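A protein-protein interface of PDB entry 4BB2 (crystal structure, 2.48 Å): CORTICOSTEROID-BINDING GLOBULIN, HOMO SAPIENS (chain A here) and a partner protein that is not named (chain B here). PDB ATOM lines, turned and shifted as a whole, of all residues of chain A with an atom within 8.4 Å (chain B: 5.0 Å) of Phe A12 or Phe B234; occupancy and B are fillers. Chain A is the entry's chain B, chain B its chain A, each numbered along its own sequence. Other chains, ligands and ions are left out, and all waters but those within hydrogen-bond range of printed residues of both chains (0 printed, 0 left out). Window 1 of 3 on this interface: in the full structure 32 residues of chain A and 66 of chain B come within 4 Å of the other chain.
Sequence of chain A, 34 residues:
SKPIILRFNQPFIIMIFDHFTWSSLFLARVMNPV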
ATOM      1  N   LEU A   6      -3.803 -19.202 -19.016  1.00  0.00           N
ATOM      2  CA  LEU A   6      -2.517 -18.583 -18.728  1.00  0.00           C
ATOM      3  C   LEU A   6      -2.663 -17.338 -17.861  1.00  0.00           C
ATOM      4  O   LEU A   6      -3.117 -16.302 -18.343  1.00  0.00           O
ATOM      5  CB  LEU A   6      -1.806 -18.218 -20.035  1.00  0.00           C
ATOM      6  CG  LEU A   6      -0.353 -17.771 -19.915  1.00  0.00           C
ATOM      7  CD1 LEU A   6       0.517 -18.888 -19.338  1.00  0.00           C
ATOM      8  CD2 LEU A   6       0.153 -17.342 -21.274  1.00  0.00           C
ATOM      9  N   ARG A   7      -2.250 -17.444 -16.596  1.00  0.00           N
ATOM     10  CA  ARG A   7      -2.369 -16.338 -15.645  1.00  0.00           C
ATOM     11  C   ARG A   7      -1.009 -15.688 -15.354  1.00  0.00           C
ATOM     12  O   ARG A   7      -0.105 -16.320 -14.789  1.00  0.00           O
ATOM     13  CB  ARG A   7      -3.043 -16.791 -14.333  1.00  0.00           C
ATOM     14  CG  ARG A   7      -4.102 -17.882 -14.475  1.00  0.00           C
ATOM     15  CD  ARG A   7      -5.293 -17.664 -13.543  1.00  0.00           C
ATOM     16  NE  ARG A   7      -5.076 -18.148 -12.181  1.00  0.00           N
ATOM     17  CZ  ARG A   7      -4.220 -19.104 -11.856  1.00  0.00           C
ATOM     18  NH1 ARG A   7      -3.495 -19.690 -12.799  1.00  0.00           N
ATOM     19  NH2 ARG A   7      -4.092 -19.475 -10.590  1.00  0.00           N
ATOM     20  N   PHE A   8      -0.867 -14.424 -15.736  1.00  0.00           N
ATOM     21  CA  PHE A   8       0.337 -13.673 -15.399  1.00  0.00           C
ATOM     22  C   PHE A   8       0.183 -13.087 -13.994  1.00  0.00           C
ATOM     23  O   PHE A   8       0.144 -11.872 -13.819  1.00  0.00           O
ATOM     24  CB  PHE A   8       0.639 -12.589 -16.443  1.00  0.00           C
ATOM     25  CG  PHE A   8       1.239 -13.122 -17.716  1.00  0.00           C
ATOM     26  CD1 PHE A   8       0.439 -13.741 -18.679  1.00  0.00           C
ATOM     27  CD2 PHE A   8       2.616 -13.029 -17.948  1.00  0.00           C
ATOM     28  CE1 PHE A   8       0.999 -14.237 -19.854  1.00  0.00           C
ATOM     29  CE2 PHE A   8       3.179 -13.525 -19.115  1.00  0.00           C
ATOM     30  CZ  PHE A   8       2.370 -14.127 -20.071  1.00  0.00           C
ATOM     31  N   ASN A   9       0.080 -13.970 -12.999  1.00  0.00           N
ATOM     32  CA  ASN A   9      -0.052 -13.567 -11.593  1.00  0.00           C
ATOM     33  C   ASN A   9       1.223 -13.798 -10.768  1.00  0.00           C
ATOM     34  O   ASN A   9       1.171 -13.919  -9.540  1.00  0.00           O
ATOM     35  CB  ASN A   9      -1.239 -14.277 -10.942  1.00  0.00           C
ATOM     36  CG  ASN A   9      -1.103 -15.789 -10.959  1.00  0.00           C
ATOM     37  OD1 ASN A   9      -0.076 -16.335 -11.359  1.00  0.00           O
ATOM     38  ND2 ASN A   9      -2.146 -16.476 -10.522  1.00  0.00           N
ATOM     39  N   GLN A  10       2.356 -13.869 -11.456  1.00  0.00           N
ATOM     40  CA  GLN A  10       3.669 -13.977 -10.815  1.00  0.00           C
ATOM     41  C   GLN A  10       4.683 -13.214 -11.663  1.00  0.00           C
ATOM     42  O   GLN A  10       4.382 -12.866 -12.813  1.00  0.00           O
ATOM     43  CB  GLN A  10       4.080 -15.456 -10.581  1.00  0.00           C
ATOM     44  CG  GLN A  10       4.019 -16.361 -11.804  1.00  0.00           C
ATOM     45  CD  GLN A  10       4.232 -17.846 -11.490  1.00  0.00           C
ATOM     46  OE1 GLN A  10       3.772 -18.362 -10.454  1.00  0.00           O
ATOM     47  NE2 GLN A  10       4.940 -18.550 -12.401  1.00  0.00           N
ATOM     48  N   PRO A  11       5.872 -12.921 -11.109  1.00  0.00           N
ATOM     49  CA  PRO A  11       6.837 -12.106 -11.852  1.00  0.00           C
ATOM     50  C   PRO A  11       7.017 -12.531 -13.312  1.00  0.00           C
ATOM     51  O   PRO A  11       7.100 -13.719 -13.608  1.00  0.00           O
ATOM     52  CB  PRO A  11       8.120 -12.302 -11.057  1.00  0.00           C
ATOM     53  CG  PRO A  11       7.637 -12.436  -9.657  1.00  0.00           C
ATOM     54  CD  PRO A  11       6.348 -13.209  -9.747  1.00  0.00           C
ATOM     55  N   PHE A  12       7.056 -11.553 -14.216  1.00  0.00           N
ATOM     56  CA  PHE A  12       7.111 -11.826 -15.652  1.00  0.00           C
ATOM     57  C   PHE A  12       7.898 -10.771 -16.415  1.00  0.00           C
ATOM     58  O   PHE A  12       8.290  -9.754 -15.852  1.00  0.00           O
ATOM     59  CB  PHE A  12       5.705 -12.059 -16.241  1.00  0.00           C
ATOM     60  CG  PHE A  12       4.806 -10.856 -16.207  1.00  0.00           C
ATOM     61  CD1 PHE A  12       4.077 -10.540 -15.071  1.00  0.00           C
ATOM     62  CD2 PHE A  12       4.651 -10.051 -17.341  1.00  0.00           C
ATOM     63  CE1 PHE A  12       3.236  -9.426 -15.059  1.00  0.00           C
ATOM     64  CE2 PHE A  12       3.823  -8.941 -17.331  1.00  0.00           C
ATOM     65  CZ  PHE A  12       3.113  -8.625 -16.191  1.00  0.00           C
ATOM     66  N   ILE A  13       8.150 -11.048 -17.693  1.00  0.00           N
ATOM     67  CA  ILE A  13       9.031 -10.248 -18.546  1.00  0.00           C
ATOM     68  C   ILE A  13       8.211  -9.709 -19.708  1.00  0.00           C
ATOM     69  O   ILE A  13       7.459 -10.467 -20.328  1.00  0.00           O
ATOM     70  CB  ILE A  13      10.203 -11.116 -19.080  1.00  0.00           C
ATOM     71  CG1 ILE A  13      11.075 -11.605 -17.917  1.00  0.00           C
ATOM     72  CG2 ILE A  13      11.052 -10.379 -20.115  1.00  0.00           C
ATOM     73  CD1 ILE A  13      11.944 -12.798 -18.246  1.00  0.00           C
ATOM     74  N   ILE A  14       8.333  -8.408 -19.980  1.00  0.00           N
ATOM     75  CA  ILE A  14       7.758  -7.803 -21.178  1.00  0.00           C
ATOM     76  C   ILE A  14       8.874  -7.330 -22.123  1.00  0.00           C
ATOM     77  O   ILE A  14       9.832  -6.658 -21.695  1.00  0.00           O
ATOM     78  CB  ILE A  14       6.843  -6.600 -20.861  1.00  0.00           C
ATOM     79  CG1 ILE A  14       5.846  -6.933 -19.742  1.00  0.00           C
ATOM     80  CG2 ILE A  14       6.122  -6.127 -22.128  1.00  0.00           C
ATOM     81  CD1 ILE A  14       4.938  -5.775 -19.360  1.00  0.00           C
ATOM     82  N   MET A  15       8.759  -7.688 -23.400  1.00  0.00           N
ATOM     83  CA  MET A  15       9.709  -7.222 -24.405  1.00  0.00           C
ATOM     84  C   MET A  15       8.938  -6.599 -25.554  1.00  0.00           C
ATOM     85  O   MET A  15       8.135  -7.267 -26.205  1.00  0.00           O
ATOM     86  CB  MET A  15      10.596  -8.363 -24.948  1.00  0.00           C
ATOM     87  CG  MET A  15      11.073  -9.377 -23.920  1.00  0.00           C
ATOM     88  SD  MET A  15      12.400 -10.437 -24.523  1.00  0.00           S
ATOM     89  CE  MET A  15      11.549 -11.595 -25.585  1.00  0.00           C
ATOM     90  N   ILE A  16       9.188  -5.321 -25.810  1.00  0.00           N
ATOM     91  CA  ILE A  16       8.508  -4.641 -26.909  1.00  0.00           C
ATOM     92  C   ILE A  16       9.467  -4.372 -28.050  1.00  0.00           C
ATOM     93  O   ILE A  16      10.511  -3.743 -27.855  1.00  0.00           O
ATOM     94  CB  ILE A  16       7.807  -3.342 -26.455  1.00  0.00           C
ATOM     95  CG1 ILE A  16       6.858  -3.659 -25.303  1.00  0.00           C
ATOM     96  CG2 ILE A  16       7.069  -2.705 -27.627  1.00  0.00           C
ATOM     97  CD1 ILE A  16       6.332  -2.444 -24.584  1.00  0.00           C
ATOM     98  N   LEU A  27      12.077  -2.917 -22.439  1.00  0.00           N
ATOM     99  CA  LEU A  27      12.288  -4.172 -21.742  1.00  0.00           C
ATOM    100  C   LEU A  27      11.854  -3.997 -20.293  1.00  0.00           C
ATOM    101  O   LEU A  27      12.223  -3.018 -19.640  1.00  0.00           O
ATOM    102  CB  LEU A  27      13.755  -4.629 -21.827  1.00  0.00           C
ATOM    103  CG  LEU A  27      14.296  -5.186 -23.156  1.00  0.00           C
ATOM    104  CD1 LEU A  27      15.806  -5.364 -23.061  1.00  0.00           C
ATOM    105  CD2 LEU A  27      13.641  -6.506 -23.568  1.00  0.00           C
ATOM    106  N   ALA A  28      11.053  -4.947 -19.817  1.00  0.00           N
ATOM    107  CA  ALA A  28      10.545  -4.916 -18.461  1.00  0.00           C
ATOM    108  C   ALA A  28      10.842  -6.196 -17.704  1.00  0.00           C
ATOM    109  O   ALA A  28      10.802  -7.297 -18.264  1.00  0.00           O
ATOM    110  CB  ALA A  28       9.048  -4.661 -18.464  1.00  0.00           C
ATOM    111  N   ARG A  29      11.159  -6.030 -16.425  1.00  0.00           N
ATOM    112  CA  ARG A  29      11.000  -7.103 -15.454  1.00  0.00           C
ATOM    113  C   ARG A  29       9.917  -6.659 -14.467  1.00  0.00           C
ATOM    114  O   ARG A  29      10.140  -5.785 -13.618  1.00  0.00           O
ATOM    115  CB  ARG A  29      12.315  -7.462 -14.741  1.00  0.00           C
ATOM    116  CG  ARG A  29      12.172  -8.682 -13.842  1.00  0.00           C
ATOM    117  CD  ARG A  29      13.441  -9.039 -13.087  1.00  0.00           C
ATOM    118  NE  ARG A  29      13.873  -7.990 -12.162  1.00  0.00           N
ATOM    119  CZ  ARG A  29      14.496  -8.216 -11.010  1.00  0.00           C
ATOM    120  NH1 ARG A  29      14.749  -9.463 -10.617  1.00  0.00           N
ATOM    121  NH2 ARG A  29      14.857  -7.197 -10.239  1.00  0.00           N
ATOM    122  N   VAL A  30       8.737  -7.255 -14.602  1.00  0.00           N
ATOM    123  CA  VAL A  30       7.619  -6.906 -13.735  1.00  0.00           C
ATOM    124  C   VAL A  30       7.623  -7.819 -12.520  1.00  0.00           C
ATOM    125  O   VAL A  30       7.182  -8.958 -12.600  1.00  0.00           O
ATOM    126  CB  VAL A  30       6.254  -7.011 -14.463  1.00  0.00           C
ATOM    127  CG1 VAL A  30       5.131  -6.473 -13.582  1.00  0.00           C
ATOM    128  CG2 VAL A  30       6.290  -6.271 -15.793  1.00  0.00           C
ATOM    129  N   MET A  31       8.134  -7.314 -11.405  1.00  0.00           N
ATOM    130  CA  MET A  31       8.067  -8.030 -10.128  1.00  0.00           C
ATOM    131  C   MET A  31       6.761  -7.719  -9.400  1.00  0.00           C
ATOM    132  O   MET A  31       6.229  -8.562  -8.680  1.00  0.00           O
ATOM    133  CB  MET A  31       9.266  -7.677  -9.237  1.00  0.00           C
ATOM    134  CG  MET A  31      10.636  -7.967  -9.855  1.00  0.00           C
ATOM    135  SD  MET A  31      11.009  -9.710 -10.193  1.00  0.00           S
ATOM    136  CE  MET A  31      10.962 -10.415  -8.539  1.00  0.00           C
ATOM    137  N   ASN A  32       6.253  -6.506  -9.600  1.00  0.00           N
ATOM    138  CA  ASN A  32       5.083  -6.012  -8.886  1.00  0.00           C
ATOM    139  C   ASN A  32       4.389  -4.955  -9.738  1.00  0.00           C
ATOM    140  O   ASN A  32       4.882  -3.837  -9.854  1.00  0.00           O
ATOM    141  CB  ASN A  32       5.512  -5.426  -7.539  1.00  0.00           C
ATOM    142  CG  ASN A  32       4.340  -5.017  -6.671  1.00  0.00           C
ATOM    143  OD1 ASN A  32       3.179  -5.163  -7.052  1.00  0.00           O
ATOM    144  ND2 ASN A  32       4.645  -4.501  -5.485  1.00  0.00           N
ATOM    145  N   PRO A  33       3.245  -5.305 -10.344  1.00  0.00           N
ATOM    146  CA  PRO A  33       2.672  -4.463 -11.405  1.00  0.00           C
ATOM    147  C   PRO A  33       1.935  -3.215 -10.908  1.00  0.00           C
ATOM    148  O   PRO A  33       1.610  -2.326 -11.698  1.00  0.00           O
ATOM    149  CB  PRO A  33       1.720  -5.413 -12.134  1.00  0.00           C
ATOM    150  CG  PRO A  33       1.345  -6.437 -11.111  1.00  0.00           C
ATOM    151  CD  PRO A  33       2.448  -6.518 -10.094  1.00  0.00           C
ATOM    152  N   TRP B 176      -3.478  -2.712 -28.930  1.00  0.00           N
ATOM    153  CA  TRP B 176      -3.652  -4.136 -29.166  1.00  0.00           C
ATOM    154  C   TRP B 176      -4.496  -4.361 -30.425  1.00  0.00           C
ATOM    155  O   TRP B 176      -5.568  -3.742 -30.596  1.00  0.00           O
ATOM    156  CB  TRP B 176      -4.392  -4.775 -28.009  1.00  0.00           C
ATOM    157  CG  TRP B 176      -3.802  -4.632 -26.655  1.00  0.00           C
ATOM    158  CD1 TRP B 176      -4.439  -4.184 -25.533  1.00  0.00           C
ATOM    159  CD2 TRP B 176      -2.484  -5.000 -26.245  1.00  0.00           C
ATOM    160  NE1 TRP B 176      -3.598  -4.225 -24.455  1.00  0.00           N
ATOM    161  CE2 TRP B 176      -2.390  -4.732 -24.861  1.00  0.00           C
ATOM    162  CE3 TRP B 176      -1.372  -5.537 -26.909  1.00  0.00           C
ATOM    163  CZ2 TRP B 176      -1.228  -4.978 -24.130  1.00  0.00           C
ATOM    164  CZ3 TRP B 176      -0.223  -5.769 -26.191  1.00  0.00           C
ATOM    165  CH2 TRP B 176      -0.154  -5.491 -24.814  1.00  0.00           C
ATOM    166  N   PHE B 190      -1.793 -11.218  -6.989  1.00  0.00           N
ATOM    167  CA  PHE B 190      -0.513 -11.268  -7.664  1.00  0.00           C
ATOM    168  C   PHE B 190       0.543 -11.713  -6.666  1.00  0.00           C
ATOM    169  O   PHE B 190       0.830 -11.012  -5.692  1.00  0.00           O
ATOM    170  CB  PHE B 190      -0.147  -9.927  -8.314  1.00  0.00           C
ATOM    171  CG  PHE B 190       1.041 -10.006  -9.230  1.00  0.00           C
ATOM    172  CD1 PHE B 190       2.335  -9.961  -8.722  1.00  0.00           C
ATOM    173  CD2 PHE B 190       0.870 -10.130 -10.614  1.00  0.00           C
ATOM    174  CE1 PHE B 190       3.432 -10.032  -9.569  1.00  0.00           C
ATOM    175  CE2 PHE B 190       1.969 -10.200 -11.462  1.00  0.00           C
ATOM    176  CZ  PHE B 190       3.248 -10.151 -10.937  1.00  0.00           C
ATOM    177  N   GLN B 220       6.475 -20.192 -20.044  1.00  0.00           N
ATOM    178  CA  GLN B 220       5.513 -20.104 -21.118  1.00  0.00           C
ATOM    179  C   GLN B 220       5.563 -18.675 -21.602  1.00  0.00           C
ATOM    180  O   GLN B 220       6.020 -17.785 -20.881  1.00  0.00           O
ATOM    181  CB  GLN B 220       4.108 -20.414 -20.632  1.00  0.00           C
ATOM    182  CG  GLN B 220       4.012 -21.648 -19.774  1.00  0.00           C
ATOM    183  CD  GLN B 220       2.677 -21.743 -19.102  1.00  0.00           C
ATOM    184  OE1 GLN B 220       1.675 -22.006 -19.750  1.00  0.00           O
ATOM    185  NE2 GLN B 220       2.650 -21.518 -17.800  1.00  0.00           N
ATOM    186  N   LEU B 221       5.108 -18.461 -22.831  1.00  0.00           N
ATOM    187  CA  LEU B 221       5.084 -17.129 -23.391  1.00  0.00           C
ATOM    188  C   LEU B 221       3.959 -16.948 -24.395  1.00  0.00           C
ATOM    189  O   LEU B 221       3.517 -17.903 -25.039  1.00  0.00           O
ATOM    190  CB  LEU B 221       6.419 -16.774 -24.041  1.00  0.00           C
ATOM    191  CG  LEU B 221       6.901 -17.565 -25.261  1.00  0.00           C
ATOM    192  CD1 LEU B 221       7.790 -16.672 -26.113  1.00  0.00           C
ATOM    193  CD2 LEU B 221       7.675 -18.820 -24.859  1.00  0.00           C
ATOM    194  N   VAL B 222       3.517 -15.699 -24.525  1.00  0.00           N
ATOM    195  CA  VAL B 222       2.670 -15.319 -25.632  1.00  0.00           C
ATOM    196  C   VAL B 222       3.286 -14.152 -26.385  1.00  0.00           C
ATOM    197  O   VAL B 222       4.117 -13.408 -25.840  1.00  0.00           O
ATOM    198  CB  VAL B 222       1.222 -14.988 -25.190  1.00  0.00           C
ATOM    199  CG1 VAL B 222       0.585 -16.205 -24.531  1.00  0.00           C
ATOM    200  CG2 VAL B 222       1.196 -13.776 -24.268  1.00  0.00           C
ATOM    201  N   MET B 224       2.023 -10.805 -28.847  1.00  0.00           N
ATOM    202  CA  MET B 224       0.885  -9.983 -29.251  1.00  0.00           C
ATOM    203  C   MET B 224       1.278  -8.768 -30.064  1.00  0.00           C
ATOM    204  O   MET B 224       2.295  -8.126 -29.797  1.00  0.00           O
ATOM    205  CB  MET B 224       0.077  -9.567 -28.039  1.00  0.00           C
ATOM    206  CG  MET B 224      -0.460 -10.772 -27.304  1.00  0.00           C
ATOM    207  SD  MET B 224      -1.605 -10.284 -26.045  1.00  0.00           S
ATOM    208  CE  MET B 224      -0.735 -10.962 -24.640  1.00  0.00           C
ATOM    209  N   VAL B 232       4.834  -7.511 -29.041  1.00  0.00           N
ATOM    210  CA  VAL B 232       5.262  -7.668 -27.658  1.00  0.00           C
ATOM    211  C   VAL B 232       5.283  -9.135 -27.243  1.00  0.00           C
ATOM    212  O   VAL B 232       4.376  -9.910 -27.584  1.00  0.00           O
ATOM    213  CB  VAL B 232       4.376  -6.829 -26.699  1.00  0.00           C
ATOM    214  CG1 VAL B 232       2.901  -7.188 -26.863  1.00  0.00           C
ATOM    215  CG2 VAL B 232       4.802  -6.992 -25.246  1.00  0.00           C
ATOM    216  N   PHE B 233       6.338  -9.507 -26.523  1.00  0.00           N
ATOM    217  CA  PHE B 233       6.439 -10.815 -25.911  1.00  0.00           C
ATOM    218  C   PHE B 233       6.175 -10.677 -24.430  1.00  0.00           C
ATOM    219  O   PHE B 233       6.800  -9.867 -23.761  1.00  0.00           O
ATOM    220  CB  PHE B 233       7.837 -11.405 -26.131  1.00  0.00           C
ATOM    221  CG  PHE B 233       8.125 -11.775 -27.564  1.00  0.00           C
ATOM    222  CD1 PHE B 233       8.690 -10.854 -28.436  1.00  0.00           C
ATOM    223  CD2 PHE B 233       7.834 -13.048 -28.038  1.00  0.00           C
ATOM    224  CE1 PHE B 233       8.960 -11.188 -29.755  1.00  0.00           C
ATOM    225  CE2 PHE B 233       8.102 -13.395 -29.355  1.00  0.00           C
ATOM    226  CZ  PHE B 233       8.663 -12.461 -30.218  1.00  0.00           C
ATOM    227  N   PHE B 234       5.230 -11.457 -23.925  1.00  0.00           N
ATOM    228  CA  PHE B 234       5.032 -11.616 -22.482  1.00  0.00           C
ATOM    229  C   PHE B 234       5.545 -13.006 -22.128  1.00  0.00           C
ATOM    230  O   PHE B 234       5.086 -14.000 -22.695  1.00  0.00           O
ATOM    231  CB  PHE B 234       3.546 -11.526 -22.109  1.00  0.00           C
ATOM    232  CG  PHE B 234       2.960 -10.144 -22.202  1.00  0.00           C
ATOM    233  CD1 PHE B 234       2.414  -9.679 -23.392  1.00  0.00           C
ATOM    234  CD2 PHE B 234       2.894  -9.328 -21.079  1.00  0.00           C
ATOM    235  CE1 PHE B 234       1.846  -8.411 -23.473  1.00  0.00           C
ATOM    236  CE2 PHE B 234       2.339  -8.061 -21.157  1.00  0.00           C
ATOM    237  CZ  PHE B 234       1.815  -7.596 -22.355  1.00  0.00           C
ATOM    238  N   ILE B 235       6.492 -13.072 -21.194  1.00  0.00           N
ATOM    239  CA  ILE B 235       7.141 -14.328 -20.804  1.00  0.00           C
ATOM    240  C   ILE B 235       6.901 -14.588 -19.324  1.00  0.00           C
ATOM    241  O   ILE B 235       7.293 -13.787 -18.474  1.00  0.00           O
ATOM    242  CB  ILE B 235       8.673 -14.313 -21.097  1.00  0.00           C
ATOM    243  CG1 ILE B 235       8.940 -14.119 -22.582  1.00  0.00           C
ATOM    244  CG2 ILE B 235       9.355 -15.606 -20.680  1.00  0.00           C
ATOM    245  CD1 ILE B 235       9.648 -12.818 -22.867  1.00  0.00           C
ATOM    246  N   LEU B 236       6.256 -15.709 -19.022  1.00  0.00           N
ATOM    247  CA  LEU B 236       6.000 -16.101 -17.637  1.00  0.00           C
ATOM    248  C   LEU B 236       6.938 -17.226 -17.192  1.00  0.00           C
ATOM    249  O   LEU B 236       6.674 -18.394 -17.480  1.00  0.00           O
ATOM    250  CB  LEU B 236       4.551 -16.542 -17.472  1.00  0.00           C
ATOM    251  CG  LEU B 236       4.190 -17.096 -16.095  1.00  0.00           C
ATOM    252  CD1 LEU B 236       4.092 -15.959 -15.097  1.00  0.00           C
ATOM    253  CD2 LEU B 236       2.892 -17.895 -16.159  1.00  0.00           C
ATOM    254  N   PRO B 237       8.036 -16.884 -16.496  1.00  0.00           N
ATOM    255  CA  PRO B 237       8.875 -17.962 -16.004  1.00  0.00           C
ATOM    256  C   PRO B 237       8.165 -18.669 -14.854  1.00  0.00           C
ATOM    257  O   PRO B 237       7.328 -18.065 -14.164  1.00  0.00           O
ATOM    258  CB  PRO B 237      10.137 -17.242 -15.507  1.00  0.00           C
ATOM    259  CG  PRO B 237      10.042 -15.837 -16.031  1.00  0.00           C
ATOM    260  CD  PRO B 237       8.586 -15.560 -16.156  1.00  0.00           C
ATOM    261  N   MET B 242      12.874 -16.923 -12.721  1.00  0.00           N
ATOM    262  CA  MET B 242      13.063 -15.671 -13.437  1.00  0.00           C
ATOM    263  C   MET B 242      14.499 -15.494 -13.955  1.00  0.00           C
ATOM    264  O   MET B 242      14.721 -15.293 -15.158  1.00  0.00           O
ATOM    265  CB  MET B 242      12.643 -14.505 -12.529  1.00  0.00           C
ATOM    266  CG  MET B 242      12.931 -13.114 -13.062  1.00  0.00           C
ATOM    267  SD  MET B 242      12.084 -12.777 -14.619  1.00  0.00           S
ATOM    268  CE  MET B 242      10.484 -12.258 -13.987  1.00  0.00           C
ATOM    269  N   ILE B 270      -3.747 -11.052 -17.794  1.00  0.00           N
ATOM    270  CA  ILE B 270      -2.556 -10.208 -17.703  1.00  0.00           C
ATOM    271  C   ILE B 270      -2.935  -8.991 -16.871  1.00  0.00           C
ATOM    272  O   ILE B 270      -3.940  -8.355 -17.146  1.00  0.00           O
ATOM    273  CB  ILE B 270      -2.053  -9.786 -19.109  1.00  0.00           C
ATOM    274  CG1 ILE B 270      -1.337 -10.957 -19.775  1.00  0.00           C
ATOM    275  CG2 ILE B 270      -1.127  -8.576 -19.023  1.00  0.00           C
ATOM    276  CD1 ILE B 270      -0.772 -10.670 -21.147  1.00  0.00           C
ATOM    277  N   PRO B 271      -2.151  -8.679 -15.829  1.00  0.00           N
ATOM    278  CA  PRO B 271      -2.544  -7.542 -14.992  1.00  0.00           C
ATOM    279  C   PRO B 271      -2.432  -6.212 -15.742  1.00  0.00           C
ATOM    280  O   PRO B 271      -1.698  -6.115 -16.725  1.00  0.00           O
ATOM    281  CB  PRO B 271      -1.529  -7.577 -13.850  1.00  0.00           C
ATOM    282  CG  PRO B 271      -0.358  -8.324 -14.384  1.00  0.00           C
ATOM    283  CD  PRO B 271      -0.909  -9.319 -15.361  1.00  0.00           C
ATOM    284  N   VAL B 273      -0.602  -2.939 -15.795  1.00  0.00           N
ATOM    285  CA  VAL B 273       0.730  -2.607 -15.286  1.00  0.00           C
ATOM    286  C   VAL B 273       0.950  -1.102 -15.396  1.00  0.00           C
ATOM    287  O   VAL B 273       0.683  -0.498 -16.439  1.00  0.00           O
ATOM    288  CB  VAL B 273       1.845  -3.373 -16.051  1.00  0.00           C
ATOM    289  CG1 VAL B 273       3.234  -2.967 -15.569  1.00  0.00           C
ATOM    290  CG2 VAL B 273       1.638  -4.883 -15.945  1.00  0.00           C
ATOM    291  N   LEU B 322       0.088   0.035 -19.041  1.00  0.00           N
ATOM    292  CA  LEU B 322      -0.504  -1.089 -19.765  1.00  0.00           C
ATOM    293  C   LEU B 322      -1.968  -1.322 -19.350  1.00  0.00           C
ATOM    294  O   LEU B 322      -2.260  -1.574 -18.172  1.00  0.00           O
ATOM    295  CB  LEU B 322       0.324  -2.336 -19.471  1.00  0.00           C
ATOM    296  CG  LEU B 322       0.258  -3.488 -20.449  1.00  0.00           C
ATOM    297  CD1 LEU B 322       1.590  -4.207 -20.444  1.00  0.00           C
ATOM    298  CD2 LEU B 322      -0.879  -4.418 -20.068  1.00  0.00           C
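Leu A6 touches Gln B220 (CD1 to OE1, 3.4 Å).
Leu B236 touches Arg A7.
CE2 of Phe B190 touches O of Phe A8, at 3.4 Å.
Gln A10 touches Phe B190.
CD1 of Ile A13 touches SD of Met B242, 3.6 Å away.
Phe B234 touches Ile A14 (CE2 to CD1, 3.9 Å).
Met A15 touches Ile B235 (CE to CD1, 3.5 Å).
Met B242 touches Arg A29 (CE to CG, 3.96 Å).
Phe B190 touches Met A31 (CE1 to O, 3.3 Å).
CA of Val B273 touches O of Pro A33 (3.7 Å).
Hydrophobic or aromatic side chains of chain B within 4 Å of the printed part of chain A: Phe B190, Val B222, Val B232, Phe B233, Phe B234, Ile B235, Leu B236, Pro B237, Met B242, Ile B270, Pro B271, Val B273 and Leu B322.
Of the 18 printed residues of chain A, 14 touch a printed residue of chain B.
Hydrophobic or aromatic side chains of chain A that line the printed part of chain B: Leu A6, Phe A8, Pro A11, Phe A12, Ile A13, Ile A14, Met A15, Ile A16 and Pro A33.
Among the printed residues, 37 pairs touch across the chains.
Among the printed residues, no Asp or Glu carboxylate lies within 4 Å of a Lys or Arg side-chain nitrogen of the other chain.
N of Phe B233 lies within hydrogen-bond range of O of Met A15 (2.9 Å).
The backbone carbonyl oxygen (O) of Ile A13 sits at hydrogen-bond distance from the backbone NH (N) of Ile B235, at 2.9 Å.
The backbone carbonyl oxygen of Pro B237 lies within hydrogen-bond range of the side-chain amide nitrogen of Gln A10 (3.0 Å).
N of Val B222 is in hydrogen-bond range of O of Phe B234 (2.9 Å).
The backbone carbonyl oxygen (O) of Val B273 sits at hydrogen-bond distance from the backbone NH (N) of Leu B322 (2.7 Å).
The backbone carbonyl oxygen of Arg A7 lies close to the side-chain amide oxygen of Asn A9, 3.4 Å away.
The backbone NH (N) of Val A30 lies within hydrogen-bond range of the backbone carbonyl oxygen (O) of Phe A12 (2.8 Å).
The backbone carbonyl oxygen (O) of Ile A14 sits at hydrogen-bond distance from the backbone NH (N) of Ala A28 (2.8 Å).
SD of Met A31 is in hydrogen-bond range of NH1 of Arg A29, 3.8 Å away.
Of chain B, only Phe B190 (3.9 Å), Phe B234 (3.9 Å), Ile B235 (3.2 Å), Met B242 (3.5 Å) and Pro B271 (3.8 Å) come within 4 Å of Phe A12.
Of the printed residues of chain A, Met B242 touches Pro A11, Phe A12, Ile A13 and Arg A29.
Of the printed residues of chain B, Gln A10 touches Phe B190, Leu B236 and Pro B237.
Of the printed residues of chain B, Phe A8 touches Phe B190 (3.4 Å), Phe B234 (3.5 Å), Ile B235 (3.9 Å), Leu B236 (3.7 Å), Ile B270 (3.5 Å) and Pro B271 (3.2 Å).
The nearest residue of chain A that does not touch Phe B234 is Met A15 (5.2 Å).
The nearest printed residue of chain A that does not touch Val B232 is Ile A13 (6.6 Å).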
